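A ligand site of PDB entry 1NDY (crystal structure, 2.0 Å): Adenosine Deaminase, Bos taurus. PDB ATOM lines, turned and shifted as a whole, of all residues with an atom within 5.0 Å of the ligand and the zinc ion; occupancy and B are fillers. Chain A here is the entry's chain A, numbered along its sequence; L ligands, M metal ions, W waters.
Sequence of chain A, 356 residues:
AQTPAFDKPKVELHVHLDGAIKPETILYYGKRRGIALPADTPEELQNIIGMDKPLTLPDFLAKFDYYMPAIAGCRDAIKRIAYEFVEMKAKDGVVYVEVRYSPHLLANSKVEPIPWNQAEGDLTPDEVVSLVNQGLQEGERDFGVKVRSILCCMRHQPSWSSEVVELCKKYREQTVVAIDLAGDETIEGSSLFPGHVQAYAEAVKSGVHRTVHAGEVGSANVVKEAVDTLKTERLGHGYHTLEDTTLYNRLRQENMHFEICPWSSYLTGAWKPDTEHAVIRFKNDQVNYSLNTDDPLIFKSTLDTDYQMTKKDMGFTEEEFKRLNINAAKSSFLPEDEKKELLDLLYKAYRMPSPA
OD1 of Asp 295 lies within hydrogen-bond range of N2 of the ligand (2.9 Å).
ND1 of His 16 sits at hydrogen-bond distance from O2 of the ligand.
The side-chain carboxylate of Asp 18 sits at hydrogen-bond distance from an oxygen (O2) of the ligand (2.7 Å).
N of Leu 105 is in hydrogen-bond range of OG of Ser 102 (3.3 Å).
The backbone carbonyl oxygen (O) of Tyr 101 lies within hydrogen-bond range of the backbone NH (N) of Cys 152 (2.9 Å).
O of Leu 105 is in hydrogen-bond range of NE1 of Trp 116 (2.7 Å).
The guanidinium group (NH2) of Arg 100 lies within hydrogen-bond range of a ring nitrogen (ND1) of His 14 (3.4 Å).
CD1 of Leu 57 touches C17 of the ligand, at 3.9 Å.
Leu 61 touches the ligand.
CZ of Phe 64 touches C2 of the ligand (3.4 Å).
CA of Tyr 101 touches O2 of the ligand, 3.6 Å away.
Ser 102 touches the ligand (N to C6, 3.96 Å).
CD1 of Leu 105 touches C10 of the ligand, 3.6 Å away.
Met 154 touches the ligand.
His 156 touches the ligand.
Gly 183 touches the ligand.
Asp 184 touches the ligand (N to C17, 3.4 Å).
Hydrophobic or aromatic side chains within 4 Å of the ligand: His 16, Leu 57, Leu 61, Phe 64, Leu 105, Met 154 and His 156.
Of the 23 residues printed, 14 come within 4 Å of the ligand.
The nearest printed residue that does not touch the ligand is Phe 60 (4.01 Å).
Four residues have an atom within 4 Å of the zinc ion: His 14, His 16, His 213 and Asp 294.
The nearest printed residue that does not touch the zinc ion is His 237 (4.1 Å).
The zinc ion is bound by NE2 of His 16 (2.0 Å).
The zinc ion is bound by water W1 (2.0 Å).
NE2 of His 14 is bound to the zinc ion (2.0 Å).
The zinc ion is bound by a ring nitrogen (NE2) of His 213 (2.2 Å).
OD2 of Asp 294 binds the zinc ion, 2.2 Å away.
The zinc ion has five donor atoms within binding distance.
Water W1 bridges the side-chain carboxylate (OD1) of Asp 294 and a ring nitrogen (NE2) of His 237.
Water W2 bridges O1 of the ligand (2.7 Å) and N of Gly 183 (2.9 Å).
Water W4 lies within hydrogen-bond range of a nitrogen (N3) of the ligand (3.0 Å) and the side-chain carboxylate (OD1) of Asp 294 (3.1 Å).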
ATOM      1  N   HIS A  14     -20.863 -24.070  -6.117  1.00  0.00           N
ATOM      2  CA  HIS A  14     -19.427 -24.156  -5.840  1.00  0.00           C
ATOM      3  C   HIS A  14     -19.269 -24.580  -4.304  1.00  0.00           C
ATOM      4  O   HIS A  14     -19.228 -23.669  -3.454  1.00  0.00           O
ATOM      5  CB  HIS A  14     -18.672 -22.796  -6.111  1.00  0.00           C
ATOM      6  CG  HIS A  14     -17.123 -23.055  -6.215  1.00  0.00           C
ATOM      7  ND1 HIS A  14     -16.386 -22.815  -7.247  1.00  0.00           N
ATOM      8  CD2 HIS A  14     -16.232 -23.495  -5.198  1.00  0.00           C
ATOM      9  CE1 HIS A  14     -15.065 -23.082  -7.010  1.00  0.00           C
ATOM     10  NE2 HIS A  14     -14.938 -23.507  -5.711  1.00  0.00           N
ATOM     11  N   HIS A  16     -17.138 -27.856  -2.237  1.00  0.00           N
ATOM     12  CA  HIS A  16     -16.454 -29.131  -2.355  1.00  0.00           C
ATOM     13  C   HIS A  16     -16.938 -30.114  -1.196  1.00  0.00           C
ATOM     14  O   HIS A  16     -16.854 -29.852   0.048  1.00  0.00           O
ATOM     15  CB  HIS A  16     -14.922 -28.824  -1.976  1.00  0.00           C
ATOM     16  CG  HIS A  16     -14.202 -27.855  -2.933  1.00  0.00           C
ATOM     17  ND1 HIS A  16     -13.340 -28.285  -3.807  1.00  0.00           N
ATOM     18  CD2 HIS A  16     -14.319 -26.464  -3.112  1.00  0.00           C
ATOM     19  CE1 HIS A  16     -12.845 -27.215  -4.554  1.00  0.00           C
ATOM     20  NE2 HIS A  16     -13.444 -26.071  -4.153  1.00  0.00           N
ATOM     21  N   ASP A  18     -15.354 -32.822   0.075  1.00  0.00           N
ATOM     22  CA  ASP A  18     -14.227 -32.933   0.971  1.00  0.00           C
ATOM     23  C   ASP A  18     -13.947 -31.772   1.836  1.00  0.00           C
ATOM     24  O   ASP A  18     -13.171 -31.899   2.785  1.00  0.00           O
ATOM     25  CB  ASP A  18     -12.952 -33.628   0.320  1.00  0.00           C
ATOM     26  CG  ASP A  18     -12.418 -32.828  -0.861  1.00  0.00           C
ATOM     27  OD1 ASP A  18     -11.341 -33.142  -1.371  1.00  0.00           O
ATOM     28  OD2 ASP A  18     -13.132 -31.938  -1.348  1.00  0.00           O
ATOM     29  N   GLY A  19     -14.559 -30.608   1.586  1.00  0.00           N
ATOM     30  CA  GLY A  19     -14.562 -29.528   2.592  1.00  0.00           C
ATOM     31  C   GLY A  19     -15.935 -29.271   3.312  1.00  0.00           C
ATOM     32  O   GLY A  19     -16.208 -28.195   3.854  1.00  0.00           O
ATOM     33  N   LEU A  57      -0.355 -21.737   2.147  1.00  0.00           N
ATOM     34  CA  LEU A  57      -0.726 -23.008   1.485  1.00  0.00           C
ATOM     35  C   LEU A  57      -0.396 -24.300   2.270  1.00  0.00           C
ATOM     36  O   LEU A  57      -1.288 -25.118   2.495  1.00  0.00           O
ATOM     37  CB  LEU A  57      -0.209 -23.158   0.051  1.00  0.00           C
ATOM     38  CG  LEU A  57      -0.848 -24.334  -0.725  1.00  0.00           C
ATOM     39  CD1 LEU A  57      -2.371 -24.181  -0.901  1.00  0.00           C
ATOM     40  CD2 LEU A  57      -0.263 -24.456  -2.183  1.00  0.00           C
ATOM     41  N   PHE A  60      -2.665 -24.699   5.097  1.00  0.00           N
ATOM     42  CA  PHE A  60      -4.091 -25.071   4.682  1.00  0.00           C
ATOM     43  C   PHE A  60      -4.279 -26.502   4.332  1.00  0.00           C
ATOM     44  O   PHE A  60      -5.187 -27.155   4.813  1.00  0.00           O
ATOM     45  CB  PHE A  60      -4.415 -24.148   3.452  1.00  0.00           C
ATOM     46  CG  PHE A  60      -5.827 -24.312   2.940  1.00  0.00           C
ATOM     47  CD1 PHE A  60      -6.919 -23.679   3.605  1.00  0.00           C
ATOM     48  CD2 PHE A  60      -6.013 -25.070   1.798  1.00  0.00           C
ATOM     49  CE1 PHE A  60      -8.212 -23.824   3.059  1.00  0.00           C
ATOM     50  CE2 PHE A  60      -7.292 -25.136   1.180  1.00  0.00           C
ATOM     51  CZ  PHE A  60      -8.372 -24.522   1.848  1.00  0.00           C
ATOM     52  N   LEU A  61      -3.383 -26.994   3.438  1.00  0.00           N
ATOM     53  CA  LEU A  61      -3.375 -28.434   3.062  1.00  0.00           C
ATOM     54  C   LEU A  61      -3.093 -29.503   4.149  1.00  0.00           C
ATOM     55  O   LEU A  61      -3.634 -30.624   4.095  1.00  0.00           O
ATOM     56  CB  LEU A  61      -2.337 -28.793   2.055  1.00  0.00           C
ATOM     57  CG  LEU A  61      -2.491 -27.862   0.896  1.00  0.00           C
ATOM     58  CD1 LEU A  61      -1.353 -28.220  -0.070  1.00  0.00           C
ATOM     59  CD2 LEU A  61      -3.880 -28.125   0.120  1.00  0.00           C
ATOM     60  N   PHE A  64      -6.301 -30.942   5.468  1.00  0.00           N
ATOM     61  CA  PHE A  64      -6.683 -32.184   4.704  1.00  0.00           C
ATOM     62  C   PHE A  64      -5.852 -33.524   5.061  1.00  0.00           C
ATOM     63  O   PHE A  64      -6.379 -34.635   5.289  1.00  0.00           O
ATOM     64  CB  PHE A  64      -6.576 -32.016   3.143  1.00  0.00           C
ATOM     65  CG  PHE A  64      -7.496 -30.911   2.621  1.00  0.00           C
ATOM     66  CD1 PHE A  64      -7.031 -29.651   2.314  1.00  0.00           C
ATOM     67  CD2 PHE A  64      -8.846 -31.249   2.428  1.00  0.00           C
ATOM     68  CE1 PHE A  64      -7.930 -28.655   1.785  1.00  0.00           C
ATOM     69  CE2 PHE A  64      -9.711 -30.342   1.751  1.00  0.00           C
ATOM     70  CZ  PHE A  64      -9.266 -29.053   1.436  1.00  0.00           C
ATOM     71  N   ARG A 100     -18.777 -30.792  -5.788  1.00  0.00           N
ATOM     72  CA  ARG A 100     -17.553 -31.251  -6.472  1.00  0.00           C
ATOM     73  C   ARG A 100     -16.481 -31.878  -5.536  1.00  0.00           C
ATOM     74  O   ARG A 100     -16.537 -31.557  -4.308  1.00  0.00           O
ATOM     75  CB  ARG A 100     -16.856 -30.039  -7.152  1.00  0.00           C
ATOM     76  CG  ARG A 100     -16.139 -29.067  -6.157  1.00  0.00           C
ATOM     77  CD  ARG A 100     -15.712 -27.686  -6.807  1.00  0.00           C
ATOM     78  NE  ARG A 100     -16.854 -27.092  -7.589  1.00  0.00           N
ATOM     79  CZ  ARG A 100     -16.756 -26.073  -8.519  1.00  0.00           C
ATOM     80  NH1 ARG A 100     -15.489 -25.770  -8.864  1.00  0.00           N
ATOM     81  NH2 ARG A 100     -17.810 -25.316  -9.091  1.00  0.00           N
ATOM     82  N   TYR A 101     -15.622 -32.801  -6.224  1.00  0.00           N
ATOM     83  CA  TYR A 101     -14.578 -33.306  -5.359  1.00  0.00           C
ATOM     84  C   TYR A 101     -13.645 -34.022  -6.346  1.00  0.00           C
ATOM     85  O   TYR A 101     -14.021 -34.273  -7.511  1.00  0.00           O
ATOM     86  CB  TYR A 101     -15.159 -34.418  -4.273  1.00  0.00           C
ATOM     87  CG  TYR A 101     -15.852 -35.573  -5.051  1.00  0.00           C
ATOM     88  CD1 TYR A 101     -15.260 -36.812  -5.233  1.00  0.00           C
ATOM     89  CD2 TYR A 101     -17.190 -35.333  -5.595  1.00  0.00           C
ATOM     90  CE1 TYR A 101     -15.781 -37.770  -6.055  1.00  0.00           C
ATOM     91  CE2 TYR A 101     -17.784 -36.376  -6.317  1.00  0.00           C
ATOM     92  CZ  TYR A 101     -17.112 -37.577  -6.508  1.00  0.00           C
ATOM     93  OH  TYR A 101     -17.691 -38.583  -7.245  1.00  0.00           O
ATOM     94  N   SER A 102     -12.412 -34.341  -5.924  1.00  0.00           N
ATOM     95  CA  SER A 102     -11.570 -35.280  -6.708  1.00  0.00           C
ATOM     96  C   SER A 102     -11.717 -36.713  -6.209  1.00  0.00           C
ATOM     97  O   SER A 102     -11.444 -36.986  -5.013  1.00  0.00           O
ATOM     98  CB  SER A 102     -10.132 -34.842  -6.461  1.00  0.00           C
ATOM     99  OG  SER A 102      -9.274 -35.954  -6.767  1.00  0.00           O
ATOM    100  N   LEU A 105      -8.677 -38.473  -4.681  1.00  0.00           N
ATOM    101  CA  LEU A 105      -8.330 -38.093  -3.303  1.00  0.00           C
ATOM    102  C   LEU A 105      -9.009 -38.887  -2.133  1.00  0.00           C
ATOM    103  O   LEU A 105      -8.777 -38.748  -0.966  1.00  0.00           O
ATOM    104  CB  LEU A 105      -8.401 -36.472  -2.963  1.00  0.00           C
ATOM    105  CG  LEU A 105      -7.439 -35.641  -3.879  1.00  0.00           C
ATOM    106  CD1 LEU A 105      -7.627 -34.163  -3.507  1.00  0.00           C
ATOM    107  CD2 LEU A 105      -5.852 -35.958  -3.541  1.00  0.00           C
ATOM    108  N   TRP A 116      -2.534 -38.948   0.858  1.00  0.00           N
ATOM    109  CA  TRP A 116      -2.642 -38.798   2.321  1.00  0.00           C
ATOM    110  C   TRP A 116      -1.810 -39.879   3.059  1.00  0.00           C
ATOM    111  O   TRP A 116      -2.229 -40.392   4.055  1.00  0.00           O
ATOM    112  CB  TRP A 116      -4.162 -38.884   2.849  1.00  0.00           C
ATOM    113  CG  TRP A 116      -5.144 -38.135   1.964  1.00  0.00           C
ATOM    114  CD1 TRP A 116      -6.236 -38.637   1.216  1.00  0.00           C
ATOM    115  CD2 TRP A 116      -5.102 -36.732   1.670  1.00  0.00           C
ATOM    116  NE1 TRP A 116      -6.820 -37.650   0.515  1.00  0.00           N
ATOM    117  CE2 TRP A 116      -6.166 -36.457   0.739  1.00  0.00           C
ATOM    118  CE3 TRP A 116      -4.292 -35.664   2.105  1.00  0.00           C
ATOM    119  CZ2 TRP A 116      -6.317 -35.192   0.213  1.00  0.00           C
ATOM    120  CZ3 TRP A 116      -4.447 -34.379   1.583  1.00  0.00           C
ATOM    121  CH2 TRP A 116      -5.470 -34.156   0.585  1.00  0.00           C
ATOM    122  N   CYS A 152     -13.190 -33.185 -10.089  1.00  0.00           N
ATOM    123  CA  CYS A 152     -12.124 -32.199 -10.149  1.00  0.00           C
ATOM    124  C   CYS A 152     -10.871 -32.948 -10.593  1.00  0.00           C
ATOM    125  O   CYS A 152     -10.428 -33.905  -9.977  1.00  0.00           O
ATOM    126  CB  CYS A 152     -11.838 -31.616  -8.753  1.00  0.00           C
ATOM    127  SG  CYS A 152     -13.195 -30.690  -7.992  1.00  0.00           S
ATOM    128  N   MET A 154      -6.812 -32.254 -10.643  1.00  0.00           N
ATOM    129  CA  MET A 154      -5.889 -31.566  -9.685  1.00  0.00           C
ATOM    130  C   MET A 154      -4.711 -30.948 -10.407  1.00  0.00           C
ATOM    131  O   MET A 154      -3.994 -31.653 -11.137  1.00  0.00           O
ATOM    132  CB  MET A 154      -5.446 -32.539  -8.560  1.00  0.00           C
ATOM    133  CG  MET A 154      -6.702 -33.091  -7.774  1.00  0.00           C
ATOM    134  SD  MET A 154      -7.589 -31.743  -6.846  1.00  0.00           S
ATOM    135  CE  MET A 154      -6.270 -30.780  -6.000  1.00  0.00           C
ATOM    136  N   HIS A 156      -1.802 -30.085  -9.649  1.00  0.00           N
ATOM    137  CA  HIS A 156      -0.403 -30.593  -9.590  1.00  0.00           C
ATOM    138  C   HIS A 156      -0.270 -32.026 -10.190  1.00  0.00           C
ATOM    139  O   HIS A 156       0.748 -32.651 -10.175  1.00  0.00           O
ATOM    140  CB  HIS A 156       0.127 -30.618  -8.127  1.00  0.00           C
ATOM    141  CG  HIS A 156      -0.737 -31.608  -7.366  1.00  0.00           C
ATOM    142  ND1 HIS A 156      -1.934 -31.224  -6.963  1.00  0.00           N
ATOM    143  CD2 HIS A 156      -0.494 -32.833  -6.747  1.00  0.00           C
ATOM    144  CE1 HIS A 156      -2.519 -32.100  -6.084  1.00  0.00           C
ATOM    145  NE2 HIS A 156      -1.584 -33.128  -5.943  1.00  0.00           N
ATOM    146  N   ALA A 182      -9.139 -27.937  -9.887  1.00  0.00           N
ATOM    147  CA  ALA A 182      -8.889 -27.386  -8.526  1.00  0.00           C
ATOM    148  C   ALA A 182      -7.406 -27.661  -8.085  1.00  0.00           C
ATOM    149  O   ALA A 182      -6.639 -28.367  -8.751  1.00  0.00           O
ATOM    150  CB  ALA A 182      -9.733 -28.200  -7.530  1.00  0.00           C
ATOM    151  N   GLY A 183      -7.062 -27.127  -6.916  1.00  0.00           N
ATOM    152  CA  GLY A 183      -5.706 -27.286  -6.234  1.00  0.00           C
ATOM    153  C   GLY A 183      -5.063 -25.934  -6.253  1.00  0.00           C
ATOM    154  O   GLY A 183      -5.680 -24.859  -6.159  1.00  0.00           O
ATOM    155  N   ASP A 184      -3.794 -26.000  -6.459  1.00  0.00           N
ATOM    156  CA  ASP A 184      -2.997 -24.751  -6.378  1.00  0.00           C
ATOM    157  C   ASP A 184      -2.898 -24.031  -7.746  1.00  0.00           C
ATOM    158  O   ASP A 184      -2.155 -24.399  -8.628  1.00  0.00           O
ATOM    159  CB  ASP A 184      -1.565 -25.143  -5.814  1.00  0.00           C
ATOM    160  CG  ASP A 184      -0.628 -23.874  -5.702  1.00  0.00           C
ATOM    161  OD1 ASP A 184       0.558 -24.043  -5.459  1.00  0.00           O
ATOM    162  OD2 ASP A 184      -1.010 -22.750  -5.942  1.00  0.00           O
ATOM    163  N   HIS A 213     -11.320 -23.398 -11.352  1.00  0.00           N
ATOM    164  CA  HIS A 213     -10.946 -22.360 -10.397  1.00  0.00           C
ATOM    165  C   HIS A 213      -9.907 -21.442 -10.937  1.00  0.00           C
ATOM    166  O   HIS A 213      -8.907 -21.965 -11.356  1.00  0.00           O
ATOM    167  CB  HIS A 213     -10.256 -23.125  -9.136  1.00  0.00           C
ATOM    168  CG  HIS A 213     -11.270 -23.794  -8.254  1.00  0.00           C
ATOM    169  ND1 HIS A 213     -11.873 -24.947  -8.529  1.00  0.00           N
ATOM    170  CD2 HIS A 213     -11.594 -23.399  -6.927  1.00  0.00           C
ATOM    171  CE1 HIS A 213     -12.505 -25.334  -7.433  1.00  0.00           C
ATOM    172  NE2 HIS A 213     -12.376 -24.449  -6.416  1.00  0.00           N
ATOM    173  N   HIS A 237     -14.562 -18.493  -8.510  1.00  0.00           N
ATOM    174  CA  HIS A 237     -14.165 -17.195  -7.959  1.00  0.00           C
ATOM    175  C   HIS A 237     -13.977 -16.174  -9.077  1.00  0.00           C
ATOM    176  O   HIS A 237     -14.761 -15.258  -9.184  1.00  0.00           O
ATOM    177  CB  HIS A 237     -12.769 -17.235  -7.162  1.00  0.00           C
ATOM    178  CG  HIS A 237     -12.920 -18.221  -6.081  1.00  0.00           C
ATOM    179  ND1 HIS A 237     -13.529 -17.982  -4.880  1.00  0.00           N
ATOM    180  CD2 HIS A 237     -12.453 -19.536  -6.109  1.00  0.00           C
ATOM    181  CE1 HIS A 237     -13.448 -19.131  -4.115  1.00  0.00           C
ATOM    182  NE2 HIS A 237     -12.771 -20.081  -4.847  1.00  0.00           N
ATOM    183  N   ASP A 294     -18.022 -22.728  -0.687  1.00  0.00           N
ATOM    184  CA  ASP A 294     -16.723 -23.442  -0.896  1.00  0.00           C
ATOM    185  C   ASP A 294     -16.415 -24.623  -0.003  1.00  0.00           C
ATOM    186  O   ASP A 294     -16.399 -25.761  -0.430  1.00  0.00           O
ATOM    187  CB  ASP A 294     -15.543 -22.383  -0.842  1.00  0.00           C
ATOM    188  CG  ASP A 294     -14.377 -22.628  -1.780  1.00  0.00           C
ATOM    189  OD1 ASP A 294     -13.291 -21.877  -1.676  1.00  0.00           O
ATOM    190  OD2 ASP A 294     -14.462 -23.616  -2.543  1.00  0.00           O
ATOM    191  N   ASP A 295     -16.103 -24.356   1.281  1.00  0.00           N
ATOM    192  CA  ASP A 295     -15.744 -25.504   2.208  1.00  0.00           C
ATOM    193  C   ASP A 295     -16.327 -25.086   3.636  1.00  0.00           C
ATOM    194  O   ASP A 295     -15.642 -24.622   4.549  1.00  0.00           O
ATOM    195  CB  ASP A 295     -14.181 -25.573   2.471  1.00  0.00           C
ATOM    196  CG  ASP A 295     -13.511 -25.892   1.153  1.00  0.00           C
ATOM    197  OD1 ASP A 295     -13.212 -27.107   0.981  1.00  0.00           O
ATOM    198  OD2 ASP A 295     -13.278 -24.950   0.328  1.00  0.00           O
HETATM  199  C1  LIG L   1      -9.900 -28.003  -2.788  1.00  0.00           C
HETATM  200  N1  LIG L   1     -10.461 -29.225  -2.343  1.00  0.00           N
HETATM  201  C2  LIG L   1     -11.263 -28.862  -1.331  1.00  0.00           C
HETATM  202  N2  LIG L   1     -11.234 -27.526  -1.076  1.00  0.00           N
HETATM  203  C3  LIG L   1     -10.353 -27.026  -2.025  1.00  0.00           C
HETATM  204  C4  LIG L   1     -10.118 -25.570  -2.075  1.00  0.00           C
HETATM  205  O1  LIG L   1      -9.158 -25.181  -2.693  1.00  0.00           O
HETATM  206  N3  LIG L   1     -10.807 -24.677  -1.331  1.00  0.00           N
HETATM  207  C5  LIG L   1     -10.024 -30.656  -2.652  1.00  0.00           C
HETATM  208  C6  LIG L   1     -10.924 -31.285  -3.888  1.00  0.00           C
HETATM  209  O2  LIG L   1     -12.368 -30.942  -3.734  1.00  0.00           O
HETATM  210  C7  LIG L   1      -8.580 -30.708  -3.133  1.00  0.00           C
HETATM  211  C8  LIG L   1      -7.662 -30.401  -1.872  1.00  0.00           C
HETATM  212  C9  LIG L   1      -6.185 -30.327  -2.272  1.00  0.00           C
HETATM  213  C10 LIG L   1      -5.442 -31.491  -2.478  1.00  0.00           C
HETATM  214  C11 LIG L   1      -4.085 -31.426  -2.898  1.00  0.00           C
HETATM  215  C12 LIG L   1      -3.516 -30.151  -3.182  1.00  0.00           C
HETATM  216  C13 LIG L   1      -4.266 -28.990  -2.969  1.00  0.00           C
HETATM  217  C14 LIG L   1      -5.622 -29.054  -2.606  1.00  0.00           C
HETATM  218  C15 LIG L   1      -3.701 -27.723  -3.320  1.00  0.00           C
HETATM  219  C16 LIG L   1      -6.374 -27.883  -2.392  1.00  0.00           C
HETATM  220  C17 LIG L   1      -4.465 -26.527  -3.136  1.00  0.00           C
HETATM  221  C18 LIG L   1      -5.826 -26.649  -2.698  1.00  0.00           C
HETATM  222 ZN    ZN M   1     -13.461 -24.132  -4.487  1.00  0.00          ZN
HETATM  223  O   HOH W   1     -12.249 -22.661  -3.859  1.00  0.00           O
HETATM  224  O   HOH W   2      -9.127 -25.906  -5.280  1.00  0.00           O
HETATM  225  O   HOH W   3      -9.356 -22.808  -4.216  1.00  0.00           O
HETATM  226  O   HOH W   4     -10.281 -21.721  -1.019  1.00  0.00           O
